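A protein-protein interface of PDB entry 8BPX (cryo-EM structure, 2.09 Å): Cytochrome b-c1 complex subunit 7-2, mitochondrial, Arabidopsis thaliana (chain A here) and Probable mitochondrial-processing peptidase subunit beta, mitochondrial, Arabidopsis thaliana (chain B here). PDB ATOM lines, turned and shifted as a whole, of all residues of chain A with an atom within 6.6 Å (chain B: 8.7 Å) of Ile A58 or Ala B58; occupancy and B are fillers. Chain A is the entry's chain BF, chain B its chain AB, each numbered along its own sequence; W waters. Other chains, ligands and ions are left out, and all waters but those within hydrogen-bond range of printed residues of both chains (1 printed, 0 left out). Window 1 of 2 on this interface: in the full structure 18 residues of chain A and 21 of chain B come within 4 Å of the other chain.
NZ of Lys B62 is in salt-bridge range of OE1 of Glu B59, 3.2 Å away.
Printed residues of chain B within 4 Å of Ile A58: Tyr B54 (3.4 Å), Ala B57 (3.6 Å) and Ala B58 (3.4 Å). Printed residues of chain A within 4 Å of Ala B58: Ile A58 (3.4 Å). No residue of chain B comes within 4 Å of Pro A55. Printed residues of chain B within 4 Å of Arg A34: Tyr B54 and Asp B55. Of the printed residues of chain B, Ser A92 touches Lys B62 (2.5 Å). Printed residues of chain A within 4 Å of Ala B57: Glu A57 and Ile A58. Of the printed residues of chain A, Asp B55 touches Arg A34. Arg A56 touches none of the printed residues of chain B. The nearest residue of chain B that does not touch Ile A58 is Ile B61 (4.5 Å). The nearest residue of chain A that does not touch Ala B58 is Tyr A93 (4.1 Å). The nearest printed residue of chain A that does not touch Lys B62 is Tyr A93 (4.5 Å).
The guanidinium group (NH2) of Arg A34 is in salt-bridge range of the side-chain carboxylate (OD1) of Asp B55 (2.7 Å). The side-chain amino group (NZ) of Lys B62 is in hydrogen-bond range of the backbone carbonyl oxygen (O) of Ser A92.
Among the printed residues, merely in contact across the chains: Arg A34 with Tyr B54 (3.6 Å), Glu A57 with Tyr B54 (3.7 Å), Glu A57 with Ala B57 (3.6 Å), Ile A58 with Tyr B54 (3.4 Å), Ile A58 with Ala B57 (3.6 Å), Ile A58 with Ala B58 (3.4 Å) and Ala A61 with Tyr B54 (3.5 Å).
Water W1 lies within hydrogen-bond range of NH1 of Arg A34 (2.7 Å), OD1 of Asp B55 (2.9 Å) and O of Ser A92 (3.4 Å).
Hydrophobic or aromatic side chains of chain A within 4 Å of the printed part of chain B: Ile A58 and Ala A61. Of the 16 printed residues of chain B, 5 touch a printed residue of chain A. Hydrophobic or aromatic side chains of chain B within 4 Å of the printed part of chain A: Tyr B54, Ala B57 and Ala B58.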
ATOM      1  N   ARG A  34      30.901  32.942   7.039  1.00  0.00           N
ATOM      2  CA  ARG A  34      29.590  33.088   6.432  1.00  0.00           C
ATOM      3  C   ARG A  34      28.928  34.355   6.947  1.00  0.00           C
ATOM      4  O   ARG A  34      29.240  34.850   8.030  1.00  0.00           O
ATOM      5  CB  ARG A  34      28.706  31.882   6.733  1.00  0.00           C
ATOM      6  CG  ARG A  34      29.398  30.553   6.575  1.00  0.00           C
ATOM      7  CD  ARG A  34      28.675  29.695   5.578  1.00  0.00           C
ATOM      8  NE  ARG A  34      29.096  28.305   5.649  1.00  0.00           N
ATOM      9  CZ  ARG A  34      28.262  27.275   5.631  1.00  0.00           C
ATOM     10  NH1 ARG A  34      26.954  27.450   5.552  1.00  0.00           N
ATOM     11  NH2 ARG A  34      28.755  26.043   5.693  1.00  0.00           N
ATOM     12  N   LEU A  54      19.330  25.150  16.841  1.00  0.00           N
ATOM     13  CA  LEU A  54      19.988  24.536  15.699  1.00  0.00           C
ATOM     14  C   LEU A  54      20.677  23.228  16.090  1.00  0.00           C
ATOM     15  O   LEU A  54      21.020  23.019  17.258  1.00  0.00           O
ATOM     16  CB  LEU A  54      21.004  25.495  15.089  1.00  0.00           C
ATOM     17  CG  LEU A  54      20.434  26.668  14.284  1.00  0.00           C
ATOM     18  CD1 LEU A  54      21.515  27.676  13.959  1.00  0.00           C
ATOM     19  CD2 LEU A  54      19.739  26.188  13.013  1.00  0.00           C
ATOM     20  N   PRO A  55      20.878  22.327  15.130  1.00  0.00           N
ATOM     21  CA  PRO A  55      21.625  21.094  15.411  1.00  0.00           C
ATOM     22  C   PRO A  55      23.069  21.375  15.805  1.00  0.00           C
ATOM     23  O   PRO A  55      23.665  22.374  15.397  1.00  0.00           O
ATOM     24  CB  PRO A  55      21.539  20.324  14.088  1.00  0.00           C
ATOM     25  CG  PRO A  55      20.300  20.831  13.448  1.00  0.00           C
ATOM     26  CD  PRO A  55      20.210  22.280  13.818  1.00  0.00           C
ATOM     27  N   ARG A  56      23.628  20.463  16.602  1.00  0.00           N
ATOM     28  CA  ARG A  56      24.920  20.697  17.238  1.00  0.00           C
ATOM     29  C   ARG A  56      26.047  20.845  16.221  1.00  0.00           C
ATOM     30  O   ARG A  56      26.934  21.686  16.391  1.00  0.00           O
ATOM     31  CB  ARG A  56      25.237  19.563  18.213  1.00  0.00           C
ATOM     32  CG  ARG A  56      26.554  19.736  18.939  1.00  0.00           C
ATOM     33  CD  ARG A  56      26.781  18.627  19.943  1.00  0.00           C
ATOM     34  NE  ARG A  56      28.033  18.782  20.672  1.00  0.00           N
ATOM     35  CZ  ARG A  56      28.379  18.062  21.729  1.00  0.00           C
ATOM     36  NH1 ARG A  56      27.593  17.111  22.207  1.00  0.00           N
ATOM     37  NH2 ARG A  56      29.542  18.302  22.325  1.00  0.00           N
ATOM     38  N   GLU A  57      26.046  20.023  15.172  1.00  0.00           N
ATOM     39  CA  GLU A  57      27.146  20.054  14.210  1.00  0.00           C
ATOM     40  C   GLU A  57      27.222  21.394  13.473  1.00  0.00           C
ATOM     41  O   GLU A  57      28.317  21.890  13.191  1.00  0.00           O
ATOM     42  CB  GLU A  57      27.039  18.889  13.219  1.00  0.00           C
ATOM     43  CG  GLU A  57      25.658  18.581  12.652  1.00  0.00           C
ATOM     44  CD  GLU A  57      24.703  17.960  13.662  1.00  0.00           C
ATOM     45  OE1 GLU A  57      25.177  17.448  14.701  1.00  0.00           O
ATOM     46  OE2 GLU A  57      23.482  17.970  13.411  1.00  0.00           O
ATOM     47  N   ILE A  58      26.073  21.999  13.175  1.00  0.00           N
ATOM     48  CA  ILE A  58      26.062  23.318  12.546  1.00  0.00           C
ATOM     49  C   ILE A  58      26.654  24.374  13.473  1.00  0.00           C
ATOM     50  O   ILE A  58      27.459  25.210  13.048  1.00  0.00           O
ATOM     51  CB  ILE A  58      24.637  23.686  12.100  1.00  0.00           C
ATOM     52  CG1 ILE A  58      24.033  22.533  11.306  1.00  0.00           C
ATOM     53  CG2 ILE A  58      24.619  24.998  11.339  1.00  0.00           C
ATOM     54  CD1 ILE A  58      22.558  22.505  11.320  1.00  0.00           C
ATOM     55  N   VAL A  59      26.266  24.355  14.748  1.00  0.00           N
ATOM     56  CA  VAL A  59      26.809  25.330  15.688  1.00  0.00           C
ATOM     57  C   VAL A  59      28.300  25.108  15.896  1.00  0.00           C
ATOM     58  O   VAL A  59      29.063  26.069  16.027  1.00  0.00           O
ATOM     59  CB  VAL A  59      26.030  25.283  17.016  1.00  0.00           C
ATOM     60  CG1 VAL A  59      26.549  26.340  17.977  1.00  0.00           C
ATOM     61  CG2 VAL A  59      24.556  25.485  16.760  1.00  0.00           C
ATOM     62  N   ASP A  60      28.744  23.851  15.918  1.00  0.00           N
ATOM     63  CA  ASP A  60      30.171  23.577  16.033  1.00  0.00           C
ATOM     64  C   ASP A  60      30.931  24.090  14.816  1.00  0.00           C
ATOM     65  O   ASP A  60      32.025  24.648  14.956  1.00  0.00           O
ATOM     66  CB  ASP A  60      30.411  22.080  16.230  1.00  0.00           C
ATOM     67  CG  ASP A  60      29.753  21.544  17.487  1.00  0.00           C
ATOM     68  OD1 ASP A  60      29.612  20.308  17.600  1.00  0.00           O
ATOM     69  OD2 ASP A  60      29.378  22.351  18.361  1.00  0.00           O
ATOM     70  N   ALA A  61      30.366  23.919  13.618  1.00  0.00           N
ATOM     71  CA  ALA A  61      30.998  24.461  12.417  1.00  0.00           C
ATOM     72  C   ALA A  61      31.072  25.982  12.473  1.00  0.00           C
ATOM     73  O   ALA A  61      32.090  26.577  12.097  1.00  0.00           O
ATOM     74  CB  ALA A  61      30.240  24.002  11.173  1.00  0.00           C
ATOM     75  N   ARG A  62      30.014  26.640  12.916  1.00  0.00           N
ATOM     76  CA  ARG A  62      29.996  28.103  13.124  1.00  0.00           C
ATOM     77  C   ARG A  62      31.106  28.515  14.087  1.00  0.00           C
ATOM     78  O   ARG A  62      31.857  29.428  13.731  1.00  0.00           O
ATOM     79  CB  ARG A  62      28.629  28.671  13.505  1.00  0.00           C
ATOM     80  CG  ARG A  62      28.642  29.927  14.355  1.00  0.00           C
ATOM     81  CD  ARG A  62      27.303  30.183  15.004  1.00  0.00           C
ATOM     82  NE  ARG A  62      27.343  31.370  15.830  1.00  0.00           N
ATOM     83  CZ  ARG A  62      26.959  32.584  15.468  1.00  0.00           C
ATOM     84  NH1 ARG A  62      26.462  32.808  14.267  1.00  0.00           N
ATOM     85  NH2 ARG A  62      27.057  33.575  16.328  1.00  0.00           N
ATOM     86  N   ASN A  63      31.190  27.842  15.206  1.00  0.00           N
ATOM     87  CA  ASN A  63      32.192  28.201  16.205  1.00  0.00           C
ATOM     88  C   ASN A  63      33.605  27.984  15.678  1.00  0.00           C
ATOM     89  O   ASN A  63      34.503  28.787  15.953  1.00  0.00           O
ATOM     90  CB  ASN A  63      31.968  27.402  17.491  1.00  0.00           C
ATOM     91  CG  ASN A  63      30.720  27.834  18.237  1.00  0.00           C
ATOM     92  OD1 ASN A  63      30.349  29.005  18.227  1.00  0.00           O
ATOM     93  ND2 ASN A  63      30.062  26.884  18.884  1.00  0.00           N
ATOM     94  N   ARG A  65      34.530  28.143  12.507  1.00  0.00           N
ATOM     95  CA  ARG A  65      34.787  29.227  11.563  1.00  0.00           C
ATOM     96  C   ARG A  65      35.089  30.526  12.299  1.00  0.00           C
ATOM     97  O   ARG A  65      35.961  31.294  11.884  1.00  0.00           O
ATOM     98  CB  ARG A  65      33.597  29.403  10.618  1.00  0.00           C
ATOM     99  CG  ARG A  65      33.491  28.337   9.544  1.00  0.00           C
ATOM    100  CD  ARG A  65      32.459  28.700   8.483  1.00  0.00           C
ATOM    101  NE  ARG A  65      31.142  28.962   9.050  1.00  0.00           N
ATOM    102  CZ  ARG A  65      30.187  28.053   9.182  1.00  0.00           C
ATOM    103  NH1 ARG A  65      30.352  26.809   8.769  1.00  0.00           N
ATOM    104  NH2 ARG A  65      29.037  28.401   9.751  1.00  0.00           N
ATOM    105  N   SER A  92      23.310  29.819   3.870  1.00  0.00           N
ATOM    106  CA  SER A  92      22.654  30.173   5.118  1.00  0.00           C
ATOM    107  C   SER A  92      22.416  28.958   6.005  1.00  0.00           C
ATOM    108  O   SER A  92      22.219  27.836   5.531  1.00  0.00           O
ATOM    109  CB  SER A  92      21.322  30.874   4.845  1.00  0.00           C
ATOM    110  OG  SER A  92      20.872  31.589   5.989  1.00  0.00           O
ATOM    111  N   TYR A  93      22.448  29.200   7.315  1.00  0.00           N
ATOM    112  CA  TYR A  93      22.029  28.215   8.303  1.00  0.00           C
ATOM    113  C   TYR A  93      21.162  28.803   9.402  1.00  0.00           C
ATOM    114  O   TYR A  93      20.647  28.038  10.221  1.00  0.00           O
ATOM    115  CB  TYR A  93      23.252  27.532   8.939  1.00  0.00           C
ATOM    116  CG  TYR A  93      24.167  28.475   9.688  1.00  0.00           C
ATOM    117  CD1 TYR A  93      23.898  28.844  11.003  1.00  0.00           C
ATOM    118  CD2 TYR A  93      25.295  29.003   9.080  1.00  0.00           C
ATOM    119  CE1 TYR A  93      24.725  29.710  11.683  1.00  0.00           C
ATOM    120  CE2 TYR A  93      26.131  29.869   9.755  1.00  0.00           C
ATOM    121  CZ  TYR A  93      25.842  30.217  11.060  1.00  0.00           C
ATOM    122  OH  TYR A  93      26.669  31.077  11.739  1.00  0.00           O
ATOM    123  N   LEU A  94      20.982  30.120   9.458  1.00  0.00           N
ATOM    124  CA  LEU A  94      20.369  30.779  10.599  1.00  0.00           C
ATOM    125  C   LEU A  94      19.091  31.536  10.279  1.00  0.00           C
ATOM    126  O   LEU A  94      18.214  31.617  11.141  1.00  0.00           O
ATOM    127  CB  LEU A  94      21.368  31.759  11.237  1.00  0.00           C
ATOM    128  CG  LEU A  94      20.911  32.480  12.504  1.00  0.00           C
ATOM    129  CD1 LEU A  94      20.655  31.488  13.631  1.00  0.00           C
ATOM    130  CD2 LEU A  94      21.931  33.512  12.917  1.00  0.00           C
ATOM    131  N   PRO B  49      25.834  21.709  -1.380  1.00  0.00           N
ATOM    132  CA  PRO B  49      25.290  21.817  -0.020  1.00  0.00           C
ATOM    133  C   PRO B  49      24.700  20.529   0.530  1.00  0.00           C
ATOM    134  O   PRO B  49      23.641  20.552   1.158  1.00  0.00           O
ATOM    135  CB  PRO B  49      24.208  22.891  -0.173  1.00  0.00           C
ATOM    136  CG  PRO B  49      23.751  22.744  -1.577  1.00  0.00           C
ATOM    137  CD  PRO B  49      24.943  22.316  -2.385  1.00  0.00           C
ATOM    138  N   HIS B  50      25.371  19.402   0.303  1.00  0.00           N
ATOM    139  CA  HIS B  50      25.099  18.182   1.048  1.00  0.00           C
ATOM    140  C   HIS B  50      26.359  17.374   1.312  1.00  0.00           C
ATOM    141  O   HIS B  50      26.264  16.290   1.896  1.00  0.00           O
ATOM    142  CB  HIS B  50      24.071  17.305   0.316  1.00  0.00           C
ATOM    143  CG  HIS B  50      22.650  17.719   0.545  1.00  0.00           C
ATOM    144  ND1 HIS B  50      21.910  17.279   1.621  1.00  0.00           N
ATOM    145  CD2 HIS B  50      21.837  18.539  -0.161  1.00  0.00           C
ATOM    146  CE1 HIS B  50      20.701  17.808   1.566  1.00  0.00           C
ATOM    147  NE2 HIS B  50      20.631  18.578   0.494  1.00  0.00           N
ATOM    148  N   MET B  52      29.492  18.394   3.046  1.00  0.00           N
ATOM    149  CA  MET B  52      29.918  18.538   4.426  1.00  0.00           C
ATOM    150  C   MET B  52      28.786  18.125   5.366  1.00  0.00           C
ATOM    151  O   MET B  52      27.620  18.431   5.104  1.00  0.00           O
ATOM    152  CB  MET B  52      30.344  19.977   4.713  1.00  0.00           C
ATOM    153  CG  MET B  52      31.580  20.419   3.943  1.00  0.00           C
ATOM    154  SD  MET B  52      32.790  19.101   3.723  1.00  0.00           S
ATOM    155  CE  MET B  52      33.870  19.380   5.120  1.00  0.00           C
ATOM    156  N   PRO B  53      29.097  17.418   6.453  1.00  0.00           N
ATOM    157  CA  PRO B  53      28.029  16.975   7.366  1.00  0.00           C
ATOM    158  C   PRO B  53      27.202  18.110   7.944  1.00  0.00           C
ATOM    159  O   PRO B  53      25.981  17.967   8.079  1.00  0.00           O
ATOM    160  CB  PRO B  53      28.798  16.223   8.462  1.00  0.00           C
ATOM    161  CG  PRO B  53      30.098  15.858   7.842  1.00  0.00           C
ATOM    162  CD  PRO B  53      30.425  16.943   6.873  1.00  0.00           C
ATOM    163  N   TYR B  54      27.824  19.240   8.282  1.00  0.00           N
ATOM    164  CA  TYR B  54      27.068  20.329   8.890  1.00  0.00           C
ATOM    165  C   TYR B  54      26.166  21.024   7.878  1.00  0.00           C
ATOM    166  O   TYR B  54      25.053  21.441   8.223  1.00  0.00           O
ATOM    167  CB  TYR B  54      28.017  21.327   9.557  1.00  0.00           C
ATOM    168  CG  TYR B  54      29.227  21.703   8.733  1.00  0.00           C
ATOM    169  CD1 TYR B  54      29.153  22.701   7.772  1.00  0.00           C
ATOM    170  CD2 TYR B  54      30.446  21.069   8.927  1.00  0.00           C
ATOM    171  CE1 TYR B  54      30.251  23.051   7.021  1.00  0.00           C
ATOM    172  CE2 TYR B  54      31.554  21.413   8.179  1.00  0.00           C
ATOM    173  CZ  TYR B  54      31.449  22.405   7.227  1.00  0.00           C
ATOM    174  OH  TYR B  54      32.545  22.757   6.479  1.00  0.00           O
ATOM    175  N   ASP B  55      26.612  21.142   6.627  1.00  0.00           N
ATOM    176  CA  ASP B  55      25.760  21.713   5.587  1.00  0.00           C
ATOM    177  C   ASP B  55      24.527  20.850   5.352  1.00  0.00           C
ATOM    178  O   ASP B  55      23.422  21.369   5.158  1.00  0.00           O
ATOM    179  CB  ASP B  55      26.554  21.878   4.293  1.00  0.00           C
ATOM    180  CG  ASP B  55      27.371  23.145   4.274  1.00  0.00           C
ATOM    181  OD1 ASP B  55      27.072  24.060   5.071  1.00  0.00           O
ATOM    182  OD2 ASP B  55      28.311  23.231   3.461  1.00  0.00           O
ATOM    183  N   HIS B  56      24.700  19.529   5.362  1.00  0.00           N
ATOM    184  CA  HIS B  56      23.572  18.620   5.179  1.00  0.00           C
ATOM    185  C   HIS B  56      22.555  18.763   6.308  1.00  0.00           C
ATOM    186  O   HIS B  56      21.340  18.801   6.063  1.00  0.00           O
ATOM    187  CB  HIS B  56      24.098  17.187   5.079  1.00  0.00           C
ATOM    188  CG  HIS B  56      23.034  16.142   5.142  1.00  0.00           C
ATOM    189  ND1 HIS B  56      22.139  15.929   4.115  1.00  0.00           N
ATOM    190  CD2 HIS B  56      22.726  15.242   6.104  1.00  0.00           C
ATOM    191  CE1 HIS B  56      21.322  14.946   4.445  1.00  0.00           C
ATOM    192  NE2 HIS B  56      21.658  14.511   5.645  1.00  0.00           N
ATOM    193  N   ALA B  57      23.033  18.856   7.550  1.00  0.00           N
ATOM    194  CA  ALA B  57      22.132  19.053   8.679  1.00  0.00           C
ATOM    195  C   ALA B  57      21.406  20.388   8.579  1.00  0.00           C
ATOM    196  O   ALA B  57      20.211  20.485   8.892  1.00  0.00           O
ATOM    197  CB  ALA B  57      22.912  18.954   9.989  1.00  0.00           C
ATOM    198  N   ALA B  58      22.116  21.431   8.139  1.00  0.00           N
ATOM    199  CA  ALA B  58      21.474  22.723   7.929  1.00  0.00           C
ATOM    200  C   ALA B  58      20.371  22.623   6.883  1.00  0.00           C
ATOM    201  O   ALA B  58      19.285  23.186   7.060  1.00  0.00           O
ATOM    202  CB  ALA B  58      22.515  23.763   7.525  1.00  0.00           C
ATOM    203  N   GLU B  59      20.633  21.904   5.788  1.00  0.00           N
ATOM    204  CA  GLU B  59      19.610  21.719   4.761  1.00  0.00           C
ATOM    205  C   GLU B  59      18.390  21.001   5.320  1.00  0.00           C
ATOM    206  O   GLU B  59      17.250  21.375   5.026  1.00  0.00           O
ATOM    207  CB  GLU B  59      20.180  20.943   3.577  1.00  0.00           C
ATOM    208  CG  GLU B  59      21.234  21.670   2.756  1.00  0.00           C
ATOM    209  CD  GLU B  59      20.706  22.902   2.047  1.00  0.00           C
ATOM    210  OE1 GLU B  59      20.463  23.926   2.712  1.00  0.00           O
ATOM    211  OE2 GLU B  59      20.527  22.844   0.813  1.00  0.00           O
ATOM    212  N   ILE B  60      18.611  19.962   6.128  1.00  0.00           N
ATOM    213  CA  ILE B  60      17.490  19.206   6.687  1.00  0.00           C
ATOM    214  C   ILE B  60      16.636  20.096   7.585  1.00  0.00           C
ATOM    215  O   ILE B  60      15.398  20.101   7.493  1.00  0.00           O
ATOM    216  CB  ILE B  60      17.998  17.966   7.442  1.00  0.00           C
ATOM    217  CG1 ILE B  60      18.323  16.843   6.465  1.00  0.00           C
ATOM    218  CG2 ILE B  60      16.964  17.482   8.441  1.00  0.00           C
ATOM    219  CD1 ILE B  60      19.125  15.753   7.081  1.00  0.00           C
ATOM    220  N   ILE B  61      17.281  20.862   8.469  1.00  0.00           N
ATOM    221  CA  ILE B  61      16.508  21.691   9.390  1.00  0.00           C
ATOM    222  C   ILE B  61      15.785  22.799   8.628  1.00  0.00           C
ATOM    223  O   ILE B  61      14.641  23.149   8.949  1.00  0.00           O
ATOM    224  CB  ILE B  61      17.405  22.236  10.523  1.00  0.00           C
ATOM    225  CG1 ILE B  61      16.554  22.781  11.671  1.00  0.00           C
ATOM    226  CG2 ILE B  61      18.342  23.325  10.037  1.00  0.00           C
ATOM    227  CD1 ILE B  61      15.369  21.915  12.025  1.00  0.00           C
ATOM    228  N   LYS B  62      16.421  23.338   7.583  1.00  0.00           N
ATOM    229  CA  LYS B  62      15.774  24.357   6.766  1.00  0.00           C
ATOM    230  C   LYS B  62      14.554  23.792   6.051  1.00  0.00           C
ATOM    231  O   LYS B  62      13.527  24.470   5.926  1.00  0.00           O
ATOM    232  CB  LYS B  62      16.775  24.933   5.765  1.00  0.00           C
ATOM    233  CG  LYS B  62      17.689  25.997   6.345  1.00  0.00           C
ATOM    234  CD  LYS B  62      18.396  26.779   5.256  1.00  0.00           C
ATOM    235  CE  LYS B  62      19.634  26.056   4.776  1.00  0.00           C
ATOM    236  NZ  LYS B  62      20.523  26.923   3.954  1.00  0.00           N
ATOM    237  N   ASN B  63      14.646  22.547   5.579  1.00  0.00           N
ATOM    238  CA  ASN B  63      13.505  21.930   4.908  1.00  0.00           C
ATOM    239  C   ASN B  63      12.356  21.694   5.879  1.00  0.00           C
ATOM    240  O   ASN B  63      11.190  21.918   5.535  1.00  0.00           O
ATOM    241  CB  ASN B  63      13.927  20.620   4.246  1.00  0.00           C
ATOM    242  CG  ASN B  63      14.749  20.844   2.997  1.00  0.00           C
ATOM    243  OD1 ASN B  63      14.688  21.905   2.382  1.00  0.00           O
ATOM    244  ND2 ASN B  63      15.491  19.825   2.588  1.00  0.00           N
ATOM    245  N   LYS B  64      12.668  21.254   7.101  1.00  0.00           N
ATOM    246  CA  LYS B  64      11.625  21.105   8.115  1.00  0.00           C
ATOM    247  C   LYS B  64      10.947  22.441   8.406  1.00  0.00           C
ATOM    248  O   LYS B  64       9.716  22.519   8.535  1.00  0.00           O
ATOM    249  CB  LYS B  64      12.226  20.516   9.390  1.00  0.00           C
ATOM    250  CG  LYS B  64      11.270  19.673  10.210  1.00  0.00           C
ATOM    251  CD  LYS B  64      11.696  19.641  11.669  1.00  0.00           C
ATOM    252  CE  LYS B  64      10.852  18.670  12.478  1.00  0.00           C
ATOM    253  NZ  LYS B  64       9.549  18.381  11.822  1.00  0.00           N
ATOM    254  N   ILE B  65      11.738  23.508   8.502  1.00  0.00           N
ATOM    255  CA  ILE B  65      11.175  24.823   8.788  1.00  0.00           C
ATOM    256  C   ILE B  65      10.277  25.283   7.642  1.00  0.00           C
ATOM    257  O   ILE B  65       9.195  25.845   7.868  1.00  0.00           O
ATOM    258  CB  ILE B  65      12.308  25.821   9.076  1.00  0.00           C
ATOM    259  CG1 ILE B  65      12.733  25.692  10.534  1.00  0.00           C
ATOM    260  CG2 ILE B  65      11.875  27.247   8.769  1.00  0.00           C
ATOM    261  CD1 ILE B  65      13.590  26.801  11.006  1.00  0.00           C
HETATM  262  O   HOH W   1      24.871  25.758   5.800  1.00  0.00           O
